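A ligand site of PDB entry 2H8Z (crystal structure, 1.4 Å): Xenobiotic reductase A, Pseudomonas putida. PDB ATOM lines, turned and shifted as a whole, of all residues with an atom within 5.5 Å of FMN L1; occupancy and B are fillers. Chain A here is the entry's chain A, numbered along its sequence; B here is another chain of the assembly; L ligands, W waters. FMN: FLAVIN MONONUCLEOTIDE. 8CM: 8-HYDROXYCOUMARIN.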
ATOM      1  N   PRO A  21       6.083  10.362   0.497  1.00  0.00           N
ATOM      2  CA  PRO A  21       7.485   9.971   0.699  1.00  0.00           C
ATOM      3  C   PRO A  21       7.790   8.631   0.077  1.00  0.00           C
ATOM      4  O   PRO A  21       6.887   7.842  -0.198  1.00  0.00           O
ATOM      5  CB  PRO A  21       7.615   9.964   2.219  1.00  0.00           C
ATOM      6  CG  PRO A  21       6.271   9.442   2.635  1.00  0.00           C
ATOM      7  CD  PRO A  21       5.308  10.205   1.736  1.00  0.00           C
ATOM      8  N   PRO A  22       9.078   8.359  -0.168  1.00  0.00           N
ATOM      9  CA  PRO A  22       9.422   7.062  -0.771  1.00  0.00           C
ATOM     10  C   PRO A  22       8.939   5.914   0.098  1.00  0.00           C
ATOM     11  O   PRO A  22       9.097   5.946   1.324  1.00  0.00           O
ATOM     12  CB  PRO A  22      10.944   7.127  -0.852  1.00  0.00           C
ATOM     13  CG  PRO A  22      11.321   8.059   0.289  1.00  0.00           C
ATOM     14  CD  PRO A  22      10.285   9.140   0.143  1.00  0.00           C
ATOM     15  N   MET A  23       8.321   4.920  -0.534  1.00  0.00           N
ATOM     16  CA  MET A  23       7.838   3.752   0.176  1.00  0.00           C
ATOM     17  C   MET A  23       8.069   2.463  -0.597  1.00  0.00           C
ATOM     18  O   MET A  23       7.343   2.148  -1.545  1.00  0.00           O
ATOM     19  CB  MET A  23       6.343   3.892   0.533  1.00  0.00           C
ATOM     20  CG  MET A  23       6.040   4.914   1.633  1.00  0.00           C
ATOM     21  SD  MET A  23       4.267   4.899   2.060  1.00  0.00           S
ATOM     22  CE  MET A  23       3.596   5.785   0.671  1.00  0.00           C
ATOM     23  N   CYS A  24       9.090   1.720  -0.172  1.00  0.00           N
ATOM     24  CA  CYS A  24       9.459   0.440  -0.768  1.00  0.00           C
ATOM     25  C   CYS A  24       8.252  -0.477  -0.865  1.00  0.00           C
ATOM     26  O   CYS A  24       7.468  -0.598   0.083  1.00  0.00           O
ATOM     27  CB  CYS A  24      10.527  -0.252   0.081  1.00  0.00           C
ATOM     28  SG  CYS A  24      12.195   0.366  -0.182  1.00  0.00           S
ATOM     29  N   GLN A  25       8.124  -1.130  -2.015  1.00  0.00           N
ATOM     30  CA  GLN A  25       7.029  -2.044  -2.280  1.00  0.00           C
ATOM     31  C   GLN A  25       7.490  -3.505  -2.265  1.00  0.00           C
ATOM     32  O   GLN A  25       6.660  -4.416  -2.150  1.00  0.00           O
ATOM     33  CB  GLN A  25       6.412  -1.719  -3.637  1.00  0.00           C
ATOM     34  CG  GLN A  25       5.801  -0.331  -3.695  1.00  0.00           C
ATOM     35  CD  GLN A  25       4.618  -0.204  -2.750  1.00  0.00           C
ATOM     36  OE1 GLN A  25       3.543  -0.746  -3.001  1.00  0.00           O
ATOM     37  NE2 GLN A  25       4.821   0.522  -1.644  1.00  0.00           N
ATOM     38  N   TYR A  26       8.795  -3.721  -2.366  1.00  0.00           N
ATOM     39  CA  TYR A  26       9.384  -5.057  -2.349  1.00  0.00           C
ATOM     40  C   TYR A  26       8.753  -5.957  -3.424  1.00  0.00           C
ATOM     41  O   TYR A  26       8.600  -7.160  -3.224  1.00  0.00           O
ATOM     42  CB  TYR A  26       9.189  -5.699  -0.976  1.00  0.00           C
ATOM     43  CG  TYR A  26       9.636  -4.797   0.165  1.00  0.00           C
ATOM     44  CD1 TYR A  26      10.972  -4.749   0.560  1.00  0.00           C
ATOM     45  CD2 TYR A  26       8.723  -3.978   0.828  1.00  0.00           C
ATOM     46  CE1 TYR A  26      11.389  -3.895   1.583  1.00  0.00           C
ATOM     47  CE2 TYR A  26       9.128  -3.121   1.844  1.00  0.00           C
ATOM     48  CZ  TYR A  26      10.465  -3.085   2.219  1.00  0.00           C
ATOM     49  OH  TYR A  26      10.863  -2.228   3.219  1.00  0.00           O
ATOM     50  N   GLU A  55       9.989   4.983  -4.297  1.00  0.00           N
ATOM     51  CA  GLU A  55      10.708   4.230  -3.271  1.00  0.00           C
ATOM     52  C   GLU A  55      12.215   4.129  -3.469  1.00  0.00           C
ATOM     53  O   GLU A  55      12.729   4.316  -4.573  1.00  0.00           O
ATOM     54  CB  GLU A  55      10.154   2.806  -3.223  1.00  0.00           C
ATOM     55  CG  GLU A  55      10.407   2.043  -4.522  1.00  0.00           C
ATOM     56  CD  GLU A  55       9.551   0.809  -4.630  1.00  0.00           C
ATOM     57  OE1 GLU A  55       9.940  -0.246  -4.093  1.00  0.00           O
ATOM     58  OE2 GLU A  55       8.469   0.897  -5.255  1.00  0.00           O
ATOM     59  N   ALA A  56      12.916   3.821  -2.381  1.00  0.00           N
ATOM     60  CA  ALA A  56      14.364   3.654  -2.409  1.00  0.00           C
ATOM     61  C   ALA A  56      14.731   2.729  -3.567  1.00  0.00           C
ATOM     62  O   ALA A  56      14.382   1.530  -3.581  1.00  0.00           O
ATOM     63  CB  ALA A  56      14.843   3.067  -1.084  1.00  0.00           C
ATOM     64  N   GLN A  98      13.871   8.389  -5.013  1.00  0.00           N
ATOM     65  CA  GLN A  98      14.903   8.324  -3.996  1.00  0.00           C
ATOM     66  C   GLN A  98      15.910   7.259  -4.429  1.00  0.00           C
ATOM     67  O   GLN A  98      15.535   6.089  -4.585  1.00  0.00           O
ATOM     68  CB  GLN A  98      14.302   7.950  -2.649  1.00  0.00           C
ATOM     69  CG  GLN A  98      15.332   7.875  -1.522  1.00  0.00           C
ATOM     70  CD  GLN A  98      14.788   7.233  -0.266  1.00  0.00           C
ATOM     71  OE1 GLN A  98      14.389   6.066  -0.270  1.00  0.00           O
ATOM     72  NE2 GLN A  98      14.784   7.979   0.829  1.00  0.00           N
ATOM     73  N   GLU A 175      16.067  12.530  -4.671  1.00  0.00           N
ATOM     74  CA  GLU A 175      16.344  12.492  -3.239  1.00  0.00           C
ATOM     75  C   GLU A 175      17.410  11.449  -2.948  1.00  0.00           C
ATOM     76  O   GLU A 175      17.216  10.257  -3.200  1.00  0.00           O
ATOM     77  CB  GLU A 175      15.074  12.152  -2.453  1.00  0.00           C
ATOM     78  CG  GLU A 175      15.270  12.177  -0.933  1.00  0.00           C
ATOM     79  CD  GLU A 175      14.042  11.692  -0.170  1.00  0.00           C
ATOM     80  OE1 GLU A 175      13.034  12.430  -0.111  1.00  0.00           O
ATOM     81  OE2 GLU A 175      14.086  10.569   0.382  1.00  0.00           O
ATOM     82  N   HIS A 177      19.288   9.072  -0.597  1.00  0.00           N
ATOM     83  CA  HIS A 177      18.951   8.411   0.670  1.00  0.00           C
ATOM     84  C   HIS A 177      20.125   8.323   1.641  1.00  0.00           C
ATOM     85  O   HIS A 177      20.845   7.329   1.659  1.00  0.00           O
ATOM     86  CB  HIS A 177      18.419   7.008   0.402  1.00  0.00           C
ATOM     87  CG  HIS A 177      17.619   6.451   1.540  1.00  0.00           C
ATOM     88  ND1 HIS A 177      17.570   7.048   2.780  1.00  0.00           N
ATOM     89  CD2 HIS A 177      16.791   5.373   1.607  1.00  0.00           C
ATOM     90  CE1 HIS A 177      16.749   6.369   3.567  1.00  0.00           C
ATOM     91  NE2 HIS A 177      16.260   5.355   2.881  1.00  0.00           N
ATOM     92  N   HIS A 180      18.151   6.603   7.719  1.00  0.00           N
ATOM     93  CA  HIS A 180      17.710   5.303   8.177  1.00  0.00           C
ATOM     94  C   HIS A 180      18.738   4.180   8.321  1.00  0.00           C
ATOM     95  O   HIS A 180      18.408   2.996   8.170  1.00  0.00           O
ATOM     96  CB  HIS A 180      16.539   4.885   7.286  1.00  0.00           C
ATOM     97  CG  HIS A 180      15.440   5.904   7.235  1.00  0.00           C
ATOM     98  ND1 HIS A 180      14.445   5.901   6.284  1.00  0.00           N
ATOM     99  CD2 HIS A 180      15.187   6.972   8.036  1.00  0.00           C
ATOM    100  CE1 HIS A 180      13.627   6.920   6.491  1.00  0.00           C
ATOM    101  NE2 HIS A 180      14.058   7.588   7.549  1.00  0.00           N
ATOM    102  N   ARG A 230      17.497  12.781   2.042  1.00  0.00           N
ATOM    103  CA  ARG A 230      16.824  12.433   3.281  1.00  0.00           C
ATOM    104  C   ARG A 230      17.995  12.144   4.213  1.00  0.00           C
ATOM    105  O   ARG A 230      18.959  11.476   3.823  1.00  0.00           O
ATOM    106  CB  ARG A 230      15.918  11.206   3.120  1.00  0.00           C
ATOM    107  CG  ARG A 230      14.943  11.085   4.285  1.00  0.00           C
ATOM    108  CD  ARG A 230      13.813  10.103   4.038  1.00  0.00           C
ATOM    109  NE  ARG A 230      12.647  10.481   4.823  1.00  0.00           N
ATOM    110  CZ  ARG A 230      11.498   9.819   4.870  1.00  0.00           C
ATOM    111  NH1 ARG A 230      11.329   8.706   4.165  1.00  0.00           N
ATOM    112  NH2 ARG A 230      10.491  10.286   5.591  1.00  0.00           N
ATOM    113  N   ALA A 300       8.093  13.422   8.183  1.00  0.00           N
ATOM    114  CA  ALA A 300       6.945  12.545   8.210  1.00  0.00           C
ATOM    115  C   ALA A 300       6.839  11.785   9.506  1.00  0.00           C
ATOM    116  O   ALA A 300       7.670  11.908  10.409  1.00  0.00           O
ATOM    117  CB  ALA A 300       7.030  11.564   7.038  1.00  0.00           C
ATOM    118  N   TRP A 301       5.772  10.983   9.550  1.00  0.00           N
ATOM    119  CA  TRP A 301       5.363  10.104  10.640  1.00  0.00           C
ATOM    120  C   TRP A 301       4.139  10.634  11.366  1.00  0.00           C
ATOM    121  O   TRP A 301       4.245  11.503  12.240  1.00  0.00           O
ATOM    122  CB  TRP A 301       6.473   9.817  11.645  1.00  0.00           C
ATOM    123  CG  TRP A 301       6.037   8.754  12.618  1.00  0.00           C
ATOM    124  CD1 TRP A 301       5.227   8.928  13.700  1.00  0.00           C
ATOM    125  CD2 TRP A 301       6.281   7.358  12.517  1.00  0.00           C
ATOM    126  NE1 TRP A 301       4.947   7.718  14.285  1.00  0.00           N
ATOM    127  CE2 TRP A 301       5.579   6.726  13.579  1.00  0.00           C
ATOM    128  CE3 TRP A 301       7.017   6.550  11.637  1.00  0.00           C
ATOM    129  CZ2 TRP A 301       5.594   5.348  13.775  1.00  0.00           C
ATOM    130  CZ3 TRP A 301       7.032   5.173  11.833  1.00  0.00           C
ATOM    131  CH2 TRP A 301       6.327   4.586  12.889  1.00  0.00           C
ATOM    132  N   GLY A 302       2.985  10.119  10.992  1.00  0.00           N
ATOM    133  CA  GLY A 302       1.737  10.522  11.629  1.00  0.00           C
ATOM    134  C   GLY A 302       1.081  11.795  11.123  1.00  0.00           C
ATOM    135  O   GLY A 302       0.191  12.315  11.795  1.00  0.00           O
ATOM    136  N   PHE A 303       1.492  12.308   9.970  1.00  0.00           N
ATOM    137  CA  PHE A 303       0.874  13.519   9.435  1.00  0.00           C
ATOM    138  C   PHE A 303      -0.374  13.205   8.610  1.00  0.00           C
ATOM    139  O   PHE A 303      -0.933  14.084   7.959  1.00  0.00           O
ATOM    140  CB  PHE A 303       1.887  14.292   8.588  1.00  0.00           C
ATOM    141  CG  PHE A 303       2.916  15.035   9.397  1.00  0.00           C
ATOM    142  CD1 PHE A 303       2.595  16.230  10.024  1.00  0.00           C
ATOM    143  CD2 PHE A 303       4.199  14.531   9.549  1.00  0.00           C
ATOM    144  CE1 PHE A 303       3.537  16.924  10.780  1.00  0.00           C
ATOM    145  CE2 PHE A 303       5.161  15.211  10.308  1.00  0.00           C
ATOM    146  CZ  PHE A 303       4.816  16.412  10.920  1.00  0.00           C
ATOM    147  N   GLY A 304      -0.812  11.946   8.651  1.00  0.00           N
ATOM    148  CA  GLY A 304      -1.996  11.529   7.920  1.00  0.00           C
ATOM    149  C   GLY A 304      -3.302  12.115   8.427  1.00  0.00           C
ATOM    150  O   GLY A 304      -4.382  11.821   7.899  1.00  0.00           O
ATOM    151  N   SER A 322       4.978  15.234   4.352  1.00  0.00           N
ATOM    152  CA  SER A 322       5.043  13.901   3.765  1.00  0.00           C
ATOM    153  C   SER A 322       4.054  12.976   4.464  1.00  0.00           C
ATOM    154  O   SER A 322       4.086  12.828   5.682  1.00  0.00           O
ATOM    155  CB  SER A 322       6.466  13.348   3.890  1.00  0.00           C
ATOM    156  OG  SER A 322       7.357  14.051   3.025  1.00  0.00           O
ATOM    157  N   VAL A 323       3.192  12.347   3.669  1.00  0.00           N
ATOM    158  CA  VAL A 323       2.165  11.439   4.176  1.00  0.00           C
ATOM    159  C   VAL A 323       2.345  10.085   3.504  1.00  0.00           C
ATOM    160  O   VAL A 323       2.099   9.950   2.302  1.00  0.00           O
ATOM    161  CB  VAL A 323       0.768  11.998   3.872  1.00  0.00           C
ATOM    162  CG1 VAL A 323      -0.306  11.055   4.401  1.00  0.00           C
ATOM    163  CG2 VAL A 323       0.623  13.377   4.495  1.00  0.00           C
ATOM    164  N   GLY A 324       2.754   9.089   4.291  1.00  0.00           N
ATOM    165  CA  GLY A 324       3.010   7.775   3.729  1.00  0.00           C
ATOM    166  C   GLY A 324       1.950   6.705   3.847  1.00  0.00           C
ATOM    167  O   GLY A 324       1.208   6.450   2.905  1.00  0.00           O
ATOM    168  N   ARG A 325       1.881   6.062   5.015  1.00  0.00           N
ATOM    169  CA  ARG A 325       0.928   4.985   5.204  1.00  0.00           C
ATOM    170  C   ARG A 325      -0.528   5.363   4.919  1.00  0.00           C
ATOM    171  O   ARG A 325      -1.297   4.521   4.449  1.00  0.00           O
ATOM    172  CB  ARG A 325       1.079   4.387   6.606  1.00  0.00           C
ATOM    173  CG  ARG A 325       2.310   3.500   6.707  1.00  0.00           C
ATOM    174  CD  ARG A 325       2.681   3.154   8.142  1.00  0.00           C
ATOM    175  NE  ARG A 325       3.089   4.334   8.893  1.00  0.00           N
ATOM    176  CZ  ARG A 325       3.498   4.306  10.156  1.00  0.00           C
ATOM    177  NH1 ARG A 325       3.550   3.162  10.814  1.00  0.00           N
ATOM    178  NH2 ARG A 325       3.819   5.437  10.771  1.00  0.00           N
ATOM    179  N   ALA A 326      -0.910   6.603   5.165  1.00  0.00           N
ATOM    180  CA  ALA A 326      -2.288   7.011   4.888  1.00  0.00           C
ATOM    181  C   ALA A 326      -2.600   6.831   3.393  1.00  0.00           C
ATOM    182  O   ALA A 326      -3.746   6.578   3.029  1.00  0.00           O
ATOM    183  CB  ALA A 326      -2.515   8.462   5.299  1.00  0.00           C
ATOM    184  N   LEU A 328      -1.294   4.456   1.530  1.00  0.00           N
ATOM    185  CA  LEU A 328      -1.359   3.023   1.217  1.00  0.00           C
ATOM    186  C   LEU A 328      -2.793   2.615   1.557  1.00  0.00           C
ATOM    187  O   LEU A 328      -3.406   1.816   0.848  1.00  0.00           O
ATOM    188  CB  LEU A 328      -0.364   2.235   2.070  1.00  0.00           C
ATOM    189  CG  LEU A 328       1.113   2.624   1.913  1.00  0.00           C
ATOM    190  CD1 LEU A 328       1.975   1.709   2.787  1.00  0.00           C
ATOM    191  CD2 LEU A 328       1.527   2.513   0.454  1.00  0.00           C
ATOM    192  N   PRO B 353       2.105  -5.608   0.137  1.00  0.00           N
ATOM    193  CA  PRO B 353       2.843  -4.343   0.159  1.00  0.00           C
ATOM    194  C   PRO B 353       2.133  -3.226   0.924  1.00  0.00           C
ATOM    195  O   PRO B 353       2.761  -2.225   1.310  1.00  0.00           O
ATOM    196  CB  PRO B 353       3.030  -4.016  -1.312  1.00  0.00           C
ATOM    197  CG  PRO B 353       3.114  -5.376  -1.939  1.00  0.00           C
ATOM    198  CD  PRO B 353       1.991  -6.117  -1.245  1.00  0.00           C
ATOM    199  N   TRP B 357       1.923  -3.146   6.527  1.00  0.00           N
ATOM    200  CA  TRP B 357       2.120  -1.897   7.248  1.00  0.00           C
ATOM    201  C   TRP B 357       0.894  -1.262   7.877  1.00  0.00           C
ATOM    202  O   TRP B 357       1.017  -0.324   8.665  1.00  0.00           O
ATOM    203  CB  TRP B 357       2.787  -0.879   6.309  1.00  0.00           C
ATOM    204  CG  TRP B 357       3.953  -1.457   5.593  1.00  0.00           C
ATOM    205  CD1 TRP B 357       3.949  -2.051   4.359  1.00  0.00           C
ATOM    206  CD2 TRP B 357       5.287  -1.587   6.094  1.00  0.00           C
ATOM    207  NE1 TRP B 357       5.199  -2.539   4.060  1.00  0.00           N
ATOM    208  CE2 TRP B 357       6.034  -2.266   5.104  1.00  0.00           C
ATOM    209  CE3 TRP B 357       5.910  -1.191   7.279  1.00  0.00           C
ATOM    210  CZ2 TRP B 357       7.394  -2.558   5.273  1.00  0.00           C
ATOM    211  CZ3 TRP B 357       7.270  -1.484   7.448  1.00  0.00           C
ATOM    212  CH2 TRP B 357       7.994  -2.158   6.443  1.00  0.00           C
HETATM  213  N1  FMN L   1      11.656   5.936   3.749  1.00  0.00           N
HETATM  214  C2  FMN L   1      12.709   6.173   2.883  1.00  0.00           C
HETATM  215  O2  FMN L   1      13.446   7.014   3.062  1.00  0.00           O
HETATM  216  N3  FMN L   1      12.808   5.237   1.691  1.00  0.00           N
HETATM  217  C4  FMN L   1      11.938   4.164   1.401  1.00  0.00           C
HETATM  218  O4  FMN L   1      12.042   3.432   0.439  1.00  0.00           O
HETATM  219  C4A FMN L   1      10.852   3.943   2.340  1.00  0.00           C
HETATM  220  N5  FMN L   1       9.959   2.937   2.180  1.00  0.00           N
HETATM  221  C5A FMN L   1       8.900   2.714   3.075  1.00  0.00           C
HETATM  222  C6  FMN L   1       7.979   1.589   2.740  1.00  0.00           C
HETATM  223  C7  FMN L   1       6.873   1.339   3.606  1.00  0.00           C
HETATM  224  C7M FMN L   1       6.089   0.248   3.155  1.00  0.00           C
HETATM  225  C8  FMN L   1       6.570   2.220   4.932  1.00  0.00           C
HETATM  226  C8M FMN L   1       5.512   2.081   5.882  1.00  0.00           C
HETATM  227  C9  FMN L   1       7.493   3.248   5.148  1.00  0.00           C
HETATM  228  C9A FMN L   1       8.669   3.581   4.279  1.00  0.00           C
HETATM  229  N10 FMN L   1       9.727   4.703   4.416  1.00  0.00           N
HETATM  230  C10 FMN L   1      10.784   4.948   3.560  1.00  0.00           C
HETATM  231  C1' FMN L   1       9.470   5.555   5.575  1.00  0.00           C
HETATM  232  C2' FMN L   1       8.266   6.516   4.987  1.00  0.00           C
HETATM  233  O2' FMN L   1       8.805   7.308   3.902  1.00  0.00           O
HETATM  234  C3' FMN L   1       7.699   7.499   5.982  1.00  0.00           C
HETATM  235  O3' FMN L   1       8.746   8.400   6.474  1.00  0.00           O
HETATM  236  C4' FMN L   1       7.081   6.704   7.168  1.00  0.00           C
HETATM  237  O4' FMN L   1       6.072   5.778   6.729  1.00  0.00           O
HETATM  238  C5' FMN L   1       6.449   7.644   8.226  1.00  0.00           C
HETATM  239  O5' FMN L   1       5.284   8.424   7.579  1.00  0.00           O
HETATM  240  P   FMN L   1       3.777   7.921   7.759  1.00  0.00           P
HETATM  241  O1P FMN L   1       3.626   6.581   7.165  1.00  0.00           O
HETATM  242  O2P FMN L   1       3.463   7.923   9.250  1.00  0.00           O
HETATM  243  O3P FMN L   1       2.983   8.966   6.985  1.00  0.00           O
HETATM  244  C5  8CM L   2      11.789   0.597   4.444  1.00  0.00           C
HETATM  245  C6  8CM L   2      12.744   0.735   3.428  1.00  0.00           C
HETATM  246  C7  8CM L   2      13.623   1.848   3.401  1.00  0.00           C
HETATM  247  C8  8CM L   2      13.546   2.835   4.408  1.00  0.00           C
HETATM  248  C1A 8CM L   2      12.581   2.699   5.455  1.00  0.00           C
HETATM  249  C4A 8CM L   2      11.698   1.577   5.471  1.00  0.00           C
HETATM  250  C4  8CM L   2      10.709   1.514   6.597  1.00  0.00           C
HETATM  251  C3  8CM L   2      10.678   2.472   7.521  1.00  0.00           C
HETATM  252  C2  8CM L   2      11.623   3.660   7.480  1.00  0.00           C
HETATM  253  O1  8CM L   2      12.568   3.724   6.413  1.00  0.00           O
HETATM  254  O2  8CM L   2      11.646   4.567   8.296  1.00  0.00           O
HETATM  255  O8  8CM L   2      14.400   3.928   4.387  1.00  0.00           O
HETATM  256  O   HOH W   1       3.482  11.358   7.998  1.00  0.00           O
HETATM  257  O   HOH W   2       0.244   8.625   6.824  1.00  0.00           O
HETATM  258  O   HOH W   3       5.623  -2.474   1.063  1.00  0.00           O
HETATM  259  O   HOH W   4       1.022   7.271  10.201  1.00  0.00           O
HETATM  260  O   HOH W   5       6.745   3.785   8.690  1.00  0.00           O
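A nitrogen (N3) of FMN L1 sits at hydrogen-bond distance from the side-chain amide oxygen (OE1) of Gln 98. The backbone NH (N) of Gly 324 lies within hydrogen-bond range of an oxygen (O3P) of FMN L1 (2.7 Å). The guanidinium group of Arg 230 sits at hydrogen-bond distance from an oxygen (O3') of FMN L1, at 2.7 Å. N of Cys 24 lies within hydrogen-bond range of N5 of FMN L1 (2.8 Å). The side-chain sulfur of Cys 24 lies within hydrogen-bond range of an oxygen (O4) of FMN L1, at 3.1 Å. An oxygen (O1P) of FMN L1 sits at hydrogen-bond distance from the backbone NH (N) of Arg 325 (2.8 Å). O1P of FMN L1 is in salt-bridge range of NE of Arg 325, 2.9 Å away. An oxygen (O2P) of FMN L1 sits at hydrogen-bond distance from the backbone NH (N) of Gly 302. The backbone carbonyl oxygen of Pro 22 lies close to an oxygen (O2') of FMN L1, at 2.9 Å. O4 of FMN L1 sits at hydrogen-bond distance from N of Ala 56. The backbone NH of Trp 301 lies within hydrogen-bond range of an oxygen (O5') of FMN L1, at 3.3 Å. A ring nitrogen (NE2) of His 177 sits at hydrogen-bond distance from an oxygen (O2) of FMN L1 (3.3 Å). A ring nitrogen (NE2) of His 177 lies within hydrogen-bond range of an oxygen (O8) of 8CM L2 (2.8 Å). A ring nitrogen (ND1) of His 180 lies within hydrogen-bond range of an oxygen (O8) of 8CM L2 (2.7 Å).
N3 of FMN L1 lies close to O8 of 8CM L2 (3.4 Å).
N of Ala 56 lies close to OE1 of Gln 98, 3.4 Å away. The side-chain carboxylate (OE2) of Glu 175 sits at hydrogen-bond distance from the side-chain amide nitrogen (NE2) of Gln 98. The backbone carbonyl oxygen of Met 23 sits at hydrogen-bond distance from the side-chain amide nitrogen of Gln 25. The backbone NH (N) of Gln 25 sits at hydrogen-bond distance from the side-chain carboxylate (OE1) of Glu 55, at 2.9 Å.
Pro 21 touches FMN L1 (CB to O2', 3.4 Å). CA of Met 23 touches N5 of FMN L1, at 3.0 Å. C of Glu 55 touches O4 of FMN L1, at 3.97 Å. His 180 touches FMN L1 (CE1 to O2, 3.4 Å). Ala 300 touches FMN L1. Val 323 touches FMN L1 (C to O3P, 3.7 Å). Trp 357 of chain B touches FMN L1. Hydrophobic or aromatic side chains that line FMN L1: Pro 21, Pro 22, Met 23, Ala 56, His 177, His 180, Ala 300, Trp 301 and Trp 357 of chain B. Within 4 Å of FMN L1: Pro 21, Pro 22, Met 23, Cys 24, Glu 55, Ala 56, Gln 98, His 177, His 180, Arg 230, Ala 300, Trp 301, Gly 302, Val 323, Gly 324, Arg 325 and Trp 357 of chain B. Along chain A the residues within 4 Å of FMN L1 span positions 21 to 325. The nearest printed residue that does not touch FMN L1 is Ser 322 (4.2 Å).
Water W4 lies within hydrogen-bond range of O2P of FMN L1 (2.7 Å) and NH2 of Arg 325 (3.4 Å). Water W2 bridges an oxygen (O3P) of FMN L1 (2.8 Å) and the backbone NH of Ala 326 (2.9 Å). Water W3 lies within hydrogen-bond range of O of Cys 24, O of Pro 353 of chain B and NE1 of Trp 357 of chain B.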
